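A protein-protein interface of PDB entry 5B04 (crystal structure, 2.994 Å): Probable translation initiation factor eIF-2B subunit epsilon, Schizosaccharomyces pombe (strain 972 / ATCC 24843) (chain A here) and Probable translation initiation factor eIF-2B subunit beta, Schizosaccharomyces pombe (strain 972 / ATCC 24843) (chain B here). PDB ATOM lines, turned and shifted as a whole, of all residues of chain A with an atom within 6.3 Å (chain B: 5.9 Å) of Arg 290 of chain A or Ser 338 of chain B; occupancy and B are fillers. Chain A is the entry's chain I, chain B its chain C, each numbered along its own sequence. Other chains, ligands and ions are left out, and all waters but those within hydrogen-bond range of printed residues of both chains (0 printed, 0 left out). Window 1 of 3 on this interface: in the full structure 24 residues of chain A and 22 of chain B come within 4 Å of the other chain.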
ATOM      1  N   ASN A 133       5.303   2.507  -6.053  1.00  0.00           N
ATOM      2  CA  ASN A 133       5.848   1.705  -4.970  1.00  0.00           C
ATOM      3  C   ASN A 133       5.179   2.075  -3.652  1.00  0.00           C
ATOM      4  O   ASN A 133       5.647   1.698  -2.578  1.00  0.00           O
ATOM      5  CB  ASN A 133       7.364   1.882  -4.870  1.00  0.00           C
ATOM      6  CG  ASN A 133       7.781   3.340  -4.855  1.00  0.00           C
ATOM      7  OD1 ASN A 133       6.942   4.240  -4.838  1.00  0.00           O
ATOM      8  ND2 ASN A 133       9.087   3.580  -4.857  1.00  0.00           N
ATOM      9  N   ASN A 269       7.523   7.967  -1.437  1.00  0.00           N
ATOM     10  CA  ASN A 269       7.324   7.147  -2.602  1.00  0.00           C
ATOM     11  C   ASN A 269       7.125   7.808  -3.925  1.00  0.00           C
ATOM     12  O   ASN A 269       7.761   8.805  -4.219  1.00  0.00           O
ATOM     13  CB  ASN A 269       6.365   6.058  -2.176  1.00  0.00           C
ATOM     14  CG  ASN A 269       6.815   5.345  -0.940  1.00  0.00           C
ATOM     15  OD1 ASN A 269       7.937   4.896  -0.855  1.00  0.00           O
ATOM     16  ND2 ASN A 269       5.926   5.213   0.014  1.00  0.00           N
ATOM     17  N   LYS A 285      11.268   8.207 -17.613  1.00  0.00           N
ATOM     18  CA  LYS A 285      12.376   8.894 -16.963  1.00  0.00           C
ATOM     19  C   LYS A 285      12.372   8.611 -15.465  1.00  0.00           C
ATOM     20  O   LYS A 285      13.398   8.259 -14.885  1.00  0.00           O
ATOM     21  CB  LYS A 285      12.297  10.401 -17.210  1.00  0.00           C
ATOM     22  CG  LYS A 285      12.553  10.827 -18.645  1.00  0.00           C
ATOM     23  CD  LYS A 285      12.163  12.282 -18.853  1.00  0.00           C
ATOM     24  CE  LYS A 285      12.734  12.836 -20.146  1.00  0.00           C
ATOM     25  NZ  LYS A 285      14.216  12.973 -20.079  1.00  0.00           N
ATOM     26  N   ASP A 286      11.201   8.763 -14.851  1.00  0.00           N
ATOM     27  CA  ASP A 286      11.042   8.573 -13.413  1.00  0.00           C
ATOM     28  C   ASP A 286      11.336   7.143 -12.973  1.00  0.00           C
ATOM     29  O   ASP A 286      11.620   6.898 -11.804  1.00  0.00           O
ATOM     30  CB  ASP A 286       9.624   8.958 -12.981  1.00  0.00           C
ATOM     31  CG  ASP A 286       9.373  10.451 -13.062  1.00  0.00           C
ATOM     32  OD1 ASP A 286      10.091  11.138 -13.818  1.00  0.00           O
ATOM     33  OD2 ASP A 286       8.454  10.936 -12.369  1.00  0.00           O
ATOM     34  N   VAL A 287      11.256   6.203 -13.910  1.00  0.00           N
ATOM     35  CA  VAL A 287      11.511   4.799 -13.610  1.00  0.00           C
ATOM     36  C   VAL A 287      13.000   4.479 -13.750  1.00  0.00           C
ATOM     37  O   VAL A 287      13.550   3.689 -12.980  1.00  0.00           O
ATOM     38  CB  VAL A 287      10.678   3.867 -14.523  1.00  0.00           C
ATOM     39  CG1 VAL A 287      11.119   2.417 -14.377  1.00  0.00           C
ATOM     40  CG2 VAL A 287       9.198   4.006 -14.203  1.00  0.00           C
ATOM     41  N   LEU A 288      13.654   5.107 -14.722  1.00  0.00           N
ATOM     42  CA  LEU A 288      15.089   4.915 -14.915  1.00  0.00           C
ATOM     43  C   LEU A 288      15.861   5.576 -13.778  1.00  0.00           C
ATOM     44  O   LEU A 288      16.901   5.076 -13.348  1.00  0.00           O
ATOM     45  CB  LEU A 288      15.536   5.459 -16.271  1.00  0.00           C
ATOM     46  CG  LEU A 288      15.621   4.400 -17.375  1.00  0.00           C
ATOM     47  CD1 LEU A 288      14.277   3.718 -17.591  1.00  0.00           C
ATOM     48  CD2 LEU A 288      16.131   5.006 -18.672  1.00  0.00           C
ATOM     49  N   SER A 289      15.354   6.706 -13.299  1.00  0.00           N
ATOM     50  CA  SER A 289      15.752   7.202 -11.992  1.00  0.00           C
ATOM     51  C   SER A 289      15.074   6.284 -10.984  1.00  0.00           C
ATOM     52  O   SER A 289      13.982   5.787 -11.236  1.00  0.00           O
ATOM     53  CB  SER A 289      15.347   8.663 -11.796  1.00  0.00           C
ATOM     54  OG  SER A 289      15.881   9.480 -12.824  1.00  0.00           O
ATOM     55  N   ARG A 290      15.709   6.048  -9.845  1.00  0.00           N
ATOM     56  CA  ARG A 290      15.277   4.970  -8.958  1.00  0.00           C
ATOM     57  C   ARG A 290      14.015   5.271  -8.141  1.00  0.00           C
ATOM     58  O   ARG A 290      13.797   4.661  -7.097  1.00  0.00           O
ATOM     59  CB  ARG A 290      16.419   4.614  -8.008  1.00  0.00           C
ATOM     60  CG  ARG A 290      17.779   4.569  -8.680  1.00  0.00           C
ATOM     61  CD  ARG A 290      17.979   3.266  -9.425  1.00  0.00           C
ATOM     62  NE  ARG A 290      18.206   2.155  -8.509  1.00  0.00           N
ATOM     63  CZ  ARG A 290      18.353   0.893  -8.892  1.00  0.00           C
ATOM     64  NH1 ARG A 290      18.292   0.584 -10.178  1.00  0.00           N
ATOM     65  NH2 ARG A 290      18.558  -0.058  -7.991  1.00  0.00           N
ATOM     66  N   TRP A 291      13.181   6.190  -8.622  1.00  0.00           N
ATOM     67  CA  TRP A 291      12.037   6.676  -7.845  1.00  0.00           C
ATOM     68  C   TRP A 291      11.011   5.602  -7.485  1.00  0.00           C
ATOM     69  O   TRP A 291      10.359   5.690  -6.444  1.00  0.00           O
ATOM     70  CB  TRP A 291      11.331   7.807  -8.597  1.00  0.00           C
ATOM     71  CG  TRP A 291      12.081   9.100  -8.567  1.00  0.00           C
ATOM     72  CD1 TRP A 291      12.808   9.649  -9.582  1.00  0.00           C
ATOM     73  CD2 TRP A 291      12.188  10.003  -7.460  1.00  0.00           C
ATOM     74  NE1 TRP A 291      13.356  10.843  -9.178  1.00  0.00           N
ATOM     75  CE2 TRP A 291      12.991  11.082  -7.880  1.00  0.00           C
ATOM     76  CE3 TRP A 291      11.682  10.006  -6.158  1.00  0.00           C
ATOM     77  CZ2 TRP A 291      13.300  12.152  -7.043  1.00  0.00           C
ATOM     78  CZ3 TRP A 291      11.989  11.070  -5.328  1.00  0.00           C
ATOM     79  CH2 TRP A 291      12.790  12.127  -5.773  1.00  0.00           C
ATOM     80  N   VAL A 292      10.862   4.595  -8.337  1.00  0.00           N
ATOM     81  CA  VAL A 292       9.844   3.574  -8.110  1.00  0.00           C
ATOM     82  C   VAL A 292      10.465   2.279  -7.585  1.00  0.00           C
ATOM     83  O   VAL A 292       9.905   1.200  -7.757  1.00  0.00           O
ATOM     84  CB  VAL A 292       9.045   3.284  -9.399  1.00  0.00           C
ATOM     85  CG1 VAL A 292       7.645   2.779  -9.061  1.00  0.00           C
ATOM     86  CG2 VAL A 292       8.954   4.537 -10.253  1.00  0.00           C
ATOM     87  N   TYR A 293      11.622   2.396  -6.939  1.00  0.00           N
ATOM     88  CA  TYR A 293      12.295   1.247  -6.334  1.00  0.00           C
ATOM     89  C   TYR A 293      11.347   0.522  -5.378  1.00  0.00           C
ATOM     90  O   TYR A 293      10.606   1.168  -4.637  1.00  0.00           O
ATOM     91  CB  TYR A 293      13.561   1.703  -5.602  1.00  0.00           C
ATOM     92  CG  TYR A 293      14.439   0.574  -5.114  1.00  0.00           C
ATOM     93  CD1 TYR A 293      15.336  -0.054  -5.970  1.00  0.00           C
ATOM     94  CD2 TYR A 293      14.370   0.132  -3.799  1.00  0.00           C
ATOM     95  CE1 TYR A 293      16.138  -1.088  -5.529  1.00  0.00           C
ATOM     96  CE2 TYR A 293      15.170  -0.901  -3.349  1.00  0.00           C
ATOM     97  CZ  TYR A 293      16.051  -1.507  -4.219  1.00  0.00           C
ATOM     98  OH  TYR A 293      16.851  -2.536  -3.777  1.00  0.00           O
ATOM     99  N   PRO A 294      11.364  -0.824  -5.382  1.00  0.00           N
ATOM    100  CA  PRO A 294      12.254  -1.738  -6.109  1.00  0.00           C
ATOM    101  C   PRO A 294      11.886  -1.967  -7.573  1.00  0.00           C
ATOM    102  O   PRO A 294      12.548  -2.760  -8.241  1.00  0.00           O
ATOM    103  CB  PRO A 294      12.109  -3.042  -5.327  1.00  0.00           C
ATOM    104  CG  PRO A 294      10.706  -3.008  -4.849  1.00  0.00           C
ATOM    105  CD  PRO A 294      10.414  -1.563  -4.530  1.00  0.00           C
ATOM    106  N   VAL A 296      12.509  -1.356 -10.650  1.00  0.00           N
ATOM    107  CA  VAL A 296      13.507  -0.829 -11.571  1.00  0.00           C
ATOM    108  C   VAL A 296      14.061  -1.993 -12.391  1.00  0.00           C
ATOM    109  O   VAL A 296      14.026  -3.134 -11.932  1.00  0.00           O
ATOM    110  CB  VAL A 296      14.648  -0.104 -10.823  1.00  0.00           C
ATOM    111  CG1 VAL A 296      14.186   1.263 -10.338  1.00  0.00           C
ATOM    112  CG2 VAL A 296      15.154  -0.955  -9.667  1.00  0.00           C
ATOM    113  N   PRO A 297      14.556  -1.714 -13.611  1.00  0.00           N
ATOM    114  CA  PRO A 297      15.071  -2.744 -14.522  1.00  0.00           C
ATOM    115  C   PRO A 297      15.983  -3.784 -13.870  1.00  0.00           C
ATOM    116  O   PRO A 297      15.823  -4.976 -14.132  1.00  0.00           O
ATOM    117  CB  PRO A 297      15.849  -1.924 -15.549  1.00  0.00           C
ATOM    118  CG  PRO A 297      15.091  -0.653 -15.629  1.00  0.00           C
ATOM    119  CD  PRO A 297      14.565  -0.381 -14.244  1.00  0.00           C
ATOM    120  N   ASP A 298      16.910  -3.343 -13.025  1.00  0.00           N
ATOM    121  CA  ASP A 298      17.896  -4.246 -12.437  1.00  0.00           C
ATOM    122  C   ASP A 298      17.307  -5.166 -11.369  1.00  0.00           C
ATOM    123  O   ASP A 298      18.015  -6.001 -10.804  1.00  0.00           O
ATOM    124  CB  ASP A 298      19.057  -3.445 -11.846  1.00  0.00           C
ATOM    125  CG  ASP A 298      18.599  -2.426 -10.829  1.00  0.00           C
ATOM    126  OD1 ASP A 298      18.071  -1.373 -11.245  1.00  0.00           O
ATOM    127  OD2 ASP A 298      18.770  -2.673  -9.616  1.00  0.00           O
ATOM    128  N   SER A 299      16.016  -5.012 -11.087  1.00  0.00           N
ATOM    129  CA  SER A 299      15.325  -5.940 -10.199  1.00  0.00           C
ATOM    130  C   SER A 299      14.965  -7.200 -10.974  1.00  0.00           C
ATOM    131  O   SER A 299      14.861  -8.285 -10.400  1.00  0.00           O
ATOM    132  CB  SER A 299      14.072  -5.302  -9.599  1.00  0.00           C
ATOM    133  OG  SER A 299      14.406  -4.212  -8.758  1.00  0.00           O
ATOM    134  N   TYR A 308      22.443  -2.298 -13.249  1.00  0.00           N
ATOM    135  CA  TYR A 308      22.582  -0.857 -13.074  1.00  0.00           C
ATOM    136  C   TYR A 308      24.041  -0.444 -13.198  1.00  0.00           C
ATOM    137  O   TYR A 308      24.939  -1.121 -12.697  1.00  0.00           O
ATOM    138  CB  TYR A 308      22.027  -0.401 -11.720  1.00  0.00           C
ATOM    139  CG  TYR A 308      22.165   1.092 -11.486  1.00  0.00           C
ATOM    140  CD1 TYR A 308      23.303   1.622 -10.886  1.00  0.00           C
ATOM    141  CD2 TYR A 308      21.163   1.971 -11.877  1.00  0.00           C
ATOM    142  CE1 TYR A 308      23.435   2.983 -10.680  1.00  0.00           C
ATOM    143  CE2 TYR A 308      21.286   3.334 -11.671  1.00  0.00           C
ATOM    144  CZ  TYR A 308      22.423   3.834 -11.073  1.00  0.00           C
ATOM    145  OH  TYR A 308      22.550   5.189 -10.867  1.00  0.00           O
ATOM    146  N   GLN A 312      22.880   6.122 -14.410  1.00  0.00           N
ATOM    147  CA  GLN A 312      21.626   5.453 -14.749  1.00  0.00           C
ATOM    148  C   GLN A 312      21.652   4.775 -16.117  1.00  0.00           C
ATOM    149  O   GLN A 312      20.781   5.011 -16.952  1.00  0.00           O
ATOM    150  CB  GLN A 312      20.466   6.450 -14.684  1.00  0.00           C
ATOM    151  CG  GLN A 312      20.249   7.050 -13.303  1.00  0.00           C
ATOM    152  CD  GLN A 312      20.337   8.562 -13.304  1.00  0.00           C
ATOM    153  OE1 GLN A 312      21.060   9.151 -14.107  1.00  0.00           O
ATOM    154  NE2 GLN A 312      19.602   9.199 -12.400  1.00  0.00           N
ATOM    155  N   TYR A 314      21.356   1.191 -17.929  1.00  0.00           N
ATOM    156  CA  TYR A 314      20.880  -0.165 -17.687  1.00  0.00           C
ATOM    157  C   TYR A 314      21.145  -1.073 -18.883  1.00  0.00           C
ATOM    158  O   TYR A 314      20.599  -0.865 -19.965  1.00  0.00           O
ATOM    159  CB  TYR A 314      19.384  -0.155 -17.360  1.00  0.00           C
ATOM    160  CG  TYR A 314      19.024   0.651 -16.130  1.00  0.00           C
ATOM    161  CD1 TYR A 314      18.873   2.030 -16.198  1.00  0.00           C
ATOM    162  CD2 TYR A 314      18.827   0.030 -14.904  1.00  0.00           C
ATOM    163  CE1 TYR A 314      18.542   2.769 -15.077  1.00  0.00           C
ATOM    164  CE2 TYR A 314      18.493   0.761 -13.778  1.00  0.00           C
ATOM    165  CZ  TYR A 314      18.352   2.129 -13.871  1.00  0.00           C
ATOM    166  OH  TYR A 314      18.021   2.860 -12.753  1.00  0.00           O
ATOM    167  N   GLN B 335      24.041  -1.650  -4.146  1.00  0.00           N
ATOM    168  CA  GLN B 335      22.689  -1.433  -4.639  1.00  0.00           C
ATOM    169  C   GLN B 335      22.259   0.003  -4.382  1.00  0.00           C
ATOM    170  O   GLN B 335      22.712   0.633  -3.427  1.00  0.00           O
ATOM    171  CB  GLN B 335      21.709  -2.406  -3.982  1.00  0.00           C
ATOM    172  CG  GLN B 335      21.986  -3.867  -4.285  1.00  0.00           C
ATOM    173  CD  GLN B 335      21.997  -4.157  -5.771  1.00  0.00           C
ATOM    174  OE1 GLN B 335      22.935  -4.761  -6.290  1.00  0.00           O
ATOM    175  NE2 GLN B 335      20.949  -3.728  -6.465  1.00  0.00           N
ATOM    176  N   LEU B 336      21.388   0.521  -5.239  1.00  0.00           N
ATOM    177  CA  LEU B 336      20.876   1.876  -5.079  1.00  0.00           C
ATOM    178  C   LEU B 336      19.371   1.864  -4.856  1.00  0.00           C
ATOM    179  O   LEU B 336      18.621   1.307  -5.657  1.00  0.00           O
ATOM    180  CB  LEU B 336      21.219   2.740  -6.296  1.00  0.00           C
ATOM    181  CG  LEU B 336      22.616   3.365  -6.379  1.00  0.00           C
ATOM    182  CD1 LEU B 336      23.695   2.317  -6.608  1.00  0.00           C
ATOM    183  CD2 LEU B 336      22.661   4.430  -7.466  1.00  0.00           C
ATOM    184  N   SER B 337      18.934   2.473  -3.760  1.00  0.00           N
ATOM    185  CA  SER B 337      17.511   2.609  -3.484  1.00  0.00           C
ATOM    186  C   SER B 337      16.968   3.858  -4.168  1.00  0.00           C
ATOM    187  O   SER B 337      17.603   4.408  -5.067  1.00  0.00           O
ATOM    188  CB  SER B 337      17.250   2.670  -1.979  1.00  0.00           C
ATOM    189  OG  SER B 337      15.864   2.796  -1.707  1.00  0.00           O
ATOM    190  N   SER B 338      15.798   4.305  -3.731  1.00  0.00           N
ATOM    191  CA  SER B 338      15.150   5.463  -4.332  1.00  0.00           C
ATOM    192  C   SER B 338      15.813   6.773  -3.918  1.00  0.00           C
ATOM    193  O   SER B 338      16.312   6.894  -2.800  1.00  0.00           O
ATOM    194  CB  SER B 338      13.667   5.490  -3.956  1.00  0.00           C
ATOM    195  OG  SER B 338      13.005   6.588  -4.561  1.00  0.00           O
ATOM    196  N   PRO B 339      15.820   7.762  -4.829  1.00  0.00           N
ATOM    197  CA  PRO B 339      16.241   9.132  -4.519  1.00  0.00           C
ATOM    198  C   PRO B 339      15.373   9.739  -3.422  1.00  0.00           C
ATOM    199  O   PRO B 339      15.767  10.708  -2.775  1.00  0.00           O
ATOM    200  CB  PRO B 339      16.037   9.870  -5.845  1.00  0.00           C
ATOM    201  CG  PRO B 339      16.129   8.811  -6.881  1.00  0.00           C
ATOM    202  CD  PRO B 339      15.512   7.598  -6.259  1.00  0.00           C
ATOM    203  N   ASP B 340      14.194   9.151  -3.240  1.00  0.00           N
ATOM    204  CA  ASP B 340      13.212   9.574  -2.248  1.00  0.00           C
ATOM    205  C   ASP B 340      13.806   9.791  -0.857  1.00  0.00           C
ATOM    206  O   ASP B 340      13.445  10.740  -0.163  1.00  0.00           O
ATOM    207  CB  ASP B 340      12.091   8.534  -2.173  1.00  0.00           C
ATOM    208  CG  ASP B 340      10.998   8.922  -1.203  1.00  0.00           C
ATOM    209  OD1 ASP B 340      10.604  10.106  -1.193  1.00  0.00           O
ATOM    210  OD2 ASP B 340      10.533   8.039  -0.451  1.00  0.00           O
ATOM    211  N   LYS B 341      14.721   8.912  -0.461  1.00  0.00           N
ATOM    212  CA  LYS B 341      15.292   8.942   0.882  1.00  0.00           C
ATOM    213  C   LYS B 341      16.215  10.138   1.108  1.00  0.00           C
ATOM    214  O   LYS B 341      16.441  10.551   2.246  1.00  0.00           O
ATOM    215  CB  LYS B 341      16.054   7.643   1.156  1.00  0.00           C
ATOM    216  CG  LYS B 341      15.206   6.388   1.019  1.00  0.00           C
ATOM    217  CD  LYS B 341      14.242   6.244   2.186  1.00  0.00           C
ATOM    218  CE  LYS B 341      13.235   5.132   1.940  1.00  0.00           C
ATOM    219  NZ  LYS B 341      12.307   5.466   0.823  1.00  0.00           N
ATOM    220  N   ILE B 342      16.744  10.693   0.022  1.00  0.00           N
ATOM    221  CA  ILE B 342      17.692  11.798   0.113  1.00  0.00           C
ATOM    222  C   ILE B 342      17.055  13.129  -0.273  1.00  0.00           C
ATOM    223  O   ILE B 342      17.051  14.078   0.512  1.00  0.00           O
ATOM    224  CB  ILE B 342      18.919  11.552  -0.783  1.00  0.00           C
ATOM    225  CG1 ILE B 342      19.722  10.358  -0.266  1.00  0.00           C
ATOM    226  CG2 ILE B 342      19.792  12.788  -0.839  1.00  0.00           C
ATOM    227  CD1 ILE B 342      21.022  10.135  -1.004  1.00  0.00           C
ATOM    228  N   ILE B 356      20.305  12.359  -8.570  1.00  0.00           N
ATOM    229  CA  ILE B 356      20.248  12.030  -7.149  1.00  0.00           C
ATOM    230  C   ILE B 356      20.486  10.539  -6.935  1.00  0.00           C
ATOM    231  O   ILE B 356      19.780   9.701  -7.493  1.00  0.00           O
ATOM    232  CB  ILE B 356      18.900  12.430  -6.513  1.00  0.00           C
ATOM    233  CG1 ILE B 356      18.742  13.954  -6.486  1.00  0.00           C
ATOM    234  CG2 ILE B 356      18.812  11.900  -5.096  1.00  0.00           C
ATOM    235  CD1 ILE B 356      18.159  14.553  -7.749  1.00  0.00           C
ATOM    236  N   ASN B 358      21.131   7.345  -4.196  1.00  0.00           N
ATOM    237  CA  ASN B 358      21.033   6.809  -2.842  1.00  0.00           C
ATOM    238  C   ASN B 358      21.430   5.339  -2.770  1.00  0.00           C
ATOM    239  O   ASN B 358      20.578   4.454  -2.852  1.00  0.00           O
ATOM    240  CB  ASN B 358      19.612   6.984  -2.301  1.00  0.00           C
ATOM    241  CG  ASN B 358      19.433   6.373  -0.922  1.00  0.00           C
ATOM    242  OD1 ASN B 358      20.361   6.354  -0.111  1.00  0.00           O
ATOM    243  ND2 ASN B 358      18.239   5.859  -0.655  1.00  0.00           N
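The backbone carbonyl oxygen (O) of Leu 336 of chain B sits at hydrogen-bond distance from the guanidinium group (NH2) of Arg 290 of chain A, at 2.7 Å. The side-chain hydroxyl of Ser 338 of chain B sits close to the backbone carbonyl oxygen of Arg 290 of chain A (3.3 Å). The backbone carbonyl oxygen (O) of Trp 291 of chain A lies within hydrogen-bond range of the side-chain hydroxyl (OG) of Ser 338 of chain B, at 3.4 Å. The backbone NH of Asn 269 of chain A is in hydrogen-bond range of the side-chain carboxylate of Asp 340 of chain B (3.2 Å).
The side-chain hydroxyl (OG) of Ser 338 of chain B lies close to the backbone NH (N) of Asp 340 of chain B, at 3.1 Å. The side-chain amide nitrogen (ND2) of Asn 358 of chain B lies within hydrogen-bond range of the backbone carbonyl oxygen (O) of Ser 338 of chain B. ND2 of Asn 133 of chain A lies within hydrogen-bond range of O of Trp 291 of chain A, at 2.9 Å. O of Tyr 293 of chain A is in hydrogen-bond range of ND2 of Asn 133 of chain A (2.9 Å). The side-chain carboxylate (OD2) of Asp 298 of chain A lies within salt-bridge range of the guanidinium group (NH2) of Arg 290 of chain A (3.1 Å). NH1 of Arg 290 of chain A lies close to OH of Tyr 314 of chain A (3.4 Å).
Ser 337 of chain B touches Arg 290 of chain A (O to CB, 3.2 Å). Arg 290 of chain A touches Pro 339 of chain B. N of Trp 291 of chain A touches CD of Pro 339 of chain B, 3.6 Å away. N of Asp 340 of chain B touches CZ3 of Trp 291 of chain A, at 3.6 Å. CE1 of Tyr 293 of chain A touches O of Leu 336 of chain B, 3.5 Å away. CD2 of Tyr 293 of chain A touches OG of Ser 337 of chain B, 3.7 Å away. Ser 338 of chain B touches Tyr 293 of chain A. Asp 298 of chain A touches Gln 335 of chain B (OD2 to NE2, 3.97 Å). Tyr 308 of chain A touches Leu 336 of chain B.
Of chain B, only Leu 336, Ser 337, Ser 338 and Pro 339 come within 4 Å of Arg 290 of chain A. Ser 338 of chain B touches just these residues of chain A: Arg 290 (3.2 Å), Trp 291 (3.4 Å) and Tyr 293 (3.9 Å). Of the printed residues of chain B, Tyr 293 of chain A touches Leu 336 (3.5 Å), Ser 337 (3.7 Å) and Ser 338 (3.9 Å). Of the printed residues of chain B, Asn 269 of chain A touches Asp 340 (3.2 Å). Printed residues of chain A within 4 Å of Asp 340 of chain B: Asn 269 (3.2 Å) and Trp 291 (3.6 Å). Gln 312 of chain A touches none of the printed residues of chain B. The nearest residue of chain A that does not touch Ser 338 of chain B is Val 292 of chain A (4.8 Å). The nearest printed residue of chain A that does not touch Asp 340 of chain B is Arg 290 of chain A (5.9 Å).
Hydrophobic or aromatic side chains of chain B within 4 Å of the printed part of chain A: Leu 336 and Pro 339. Of the 19 printed residues of chain A, 6 touch a printed residue of chain B. Hydrophobic or aromatic side chains of chain A that line the printed part of chain B: Trp 291, Tyr 293 and Tyr 308. Among the printed residues, 13 pairs touch across the chains. Among the printed residues, no Asp or Glu carboxylate lies within 4 Å of a Lys or Arg side-chain nitrogen of the other chain.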
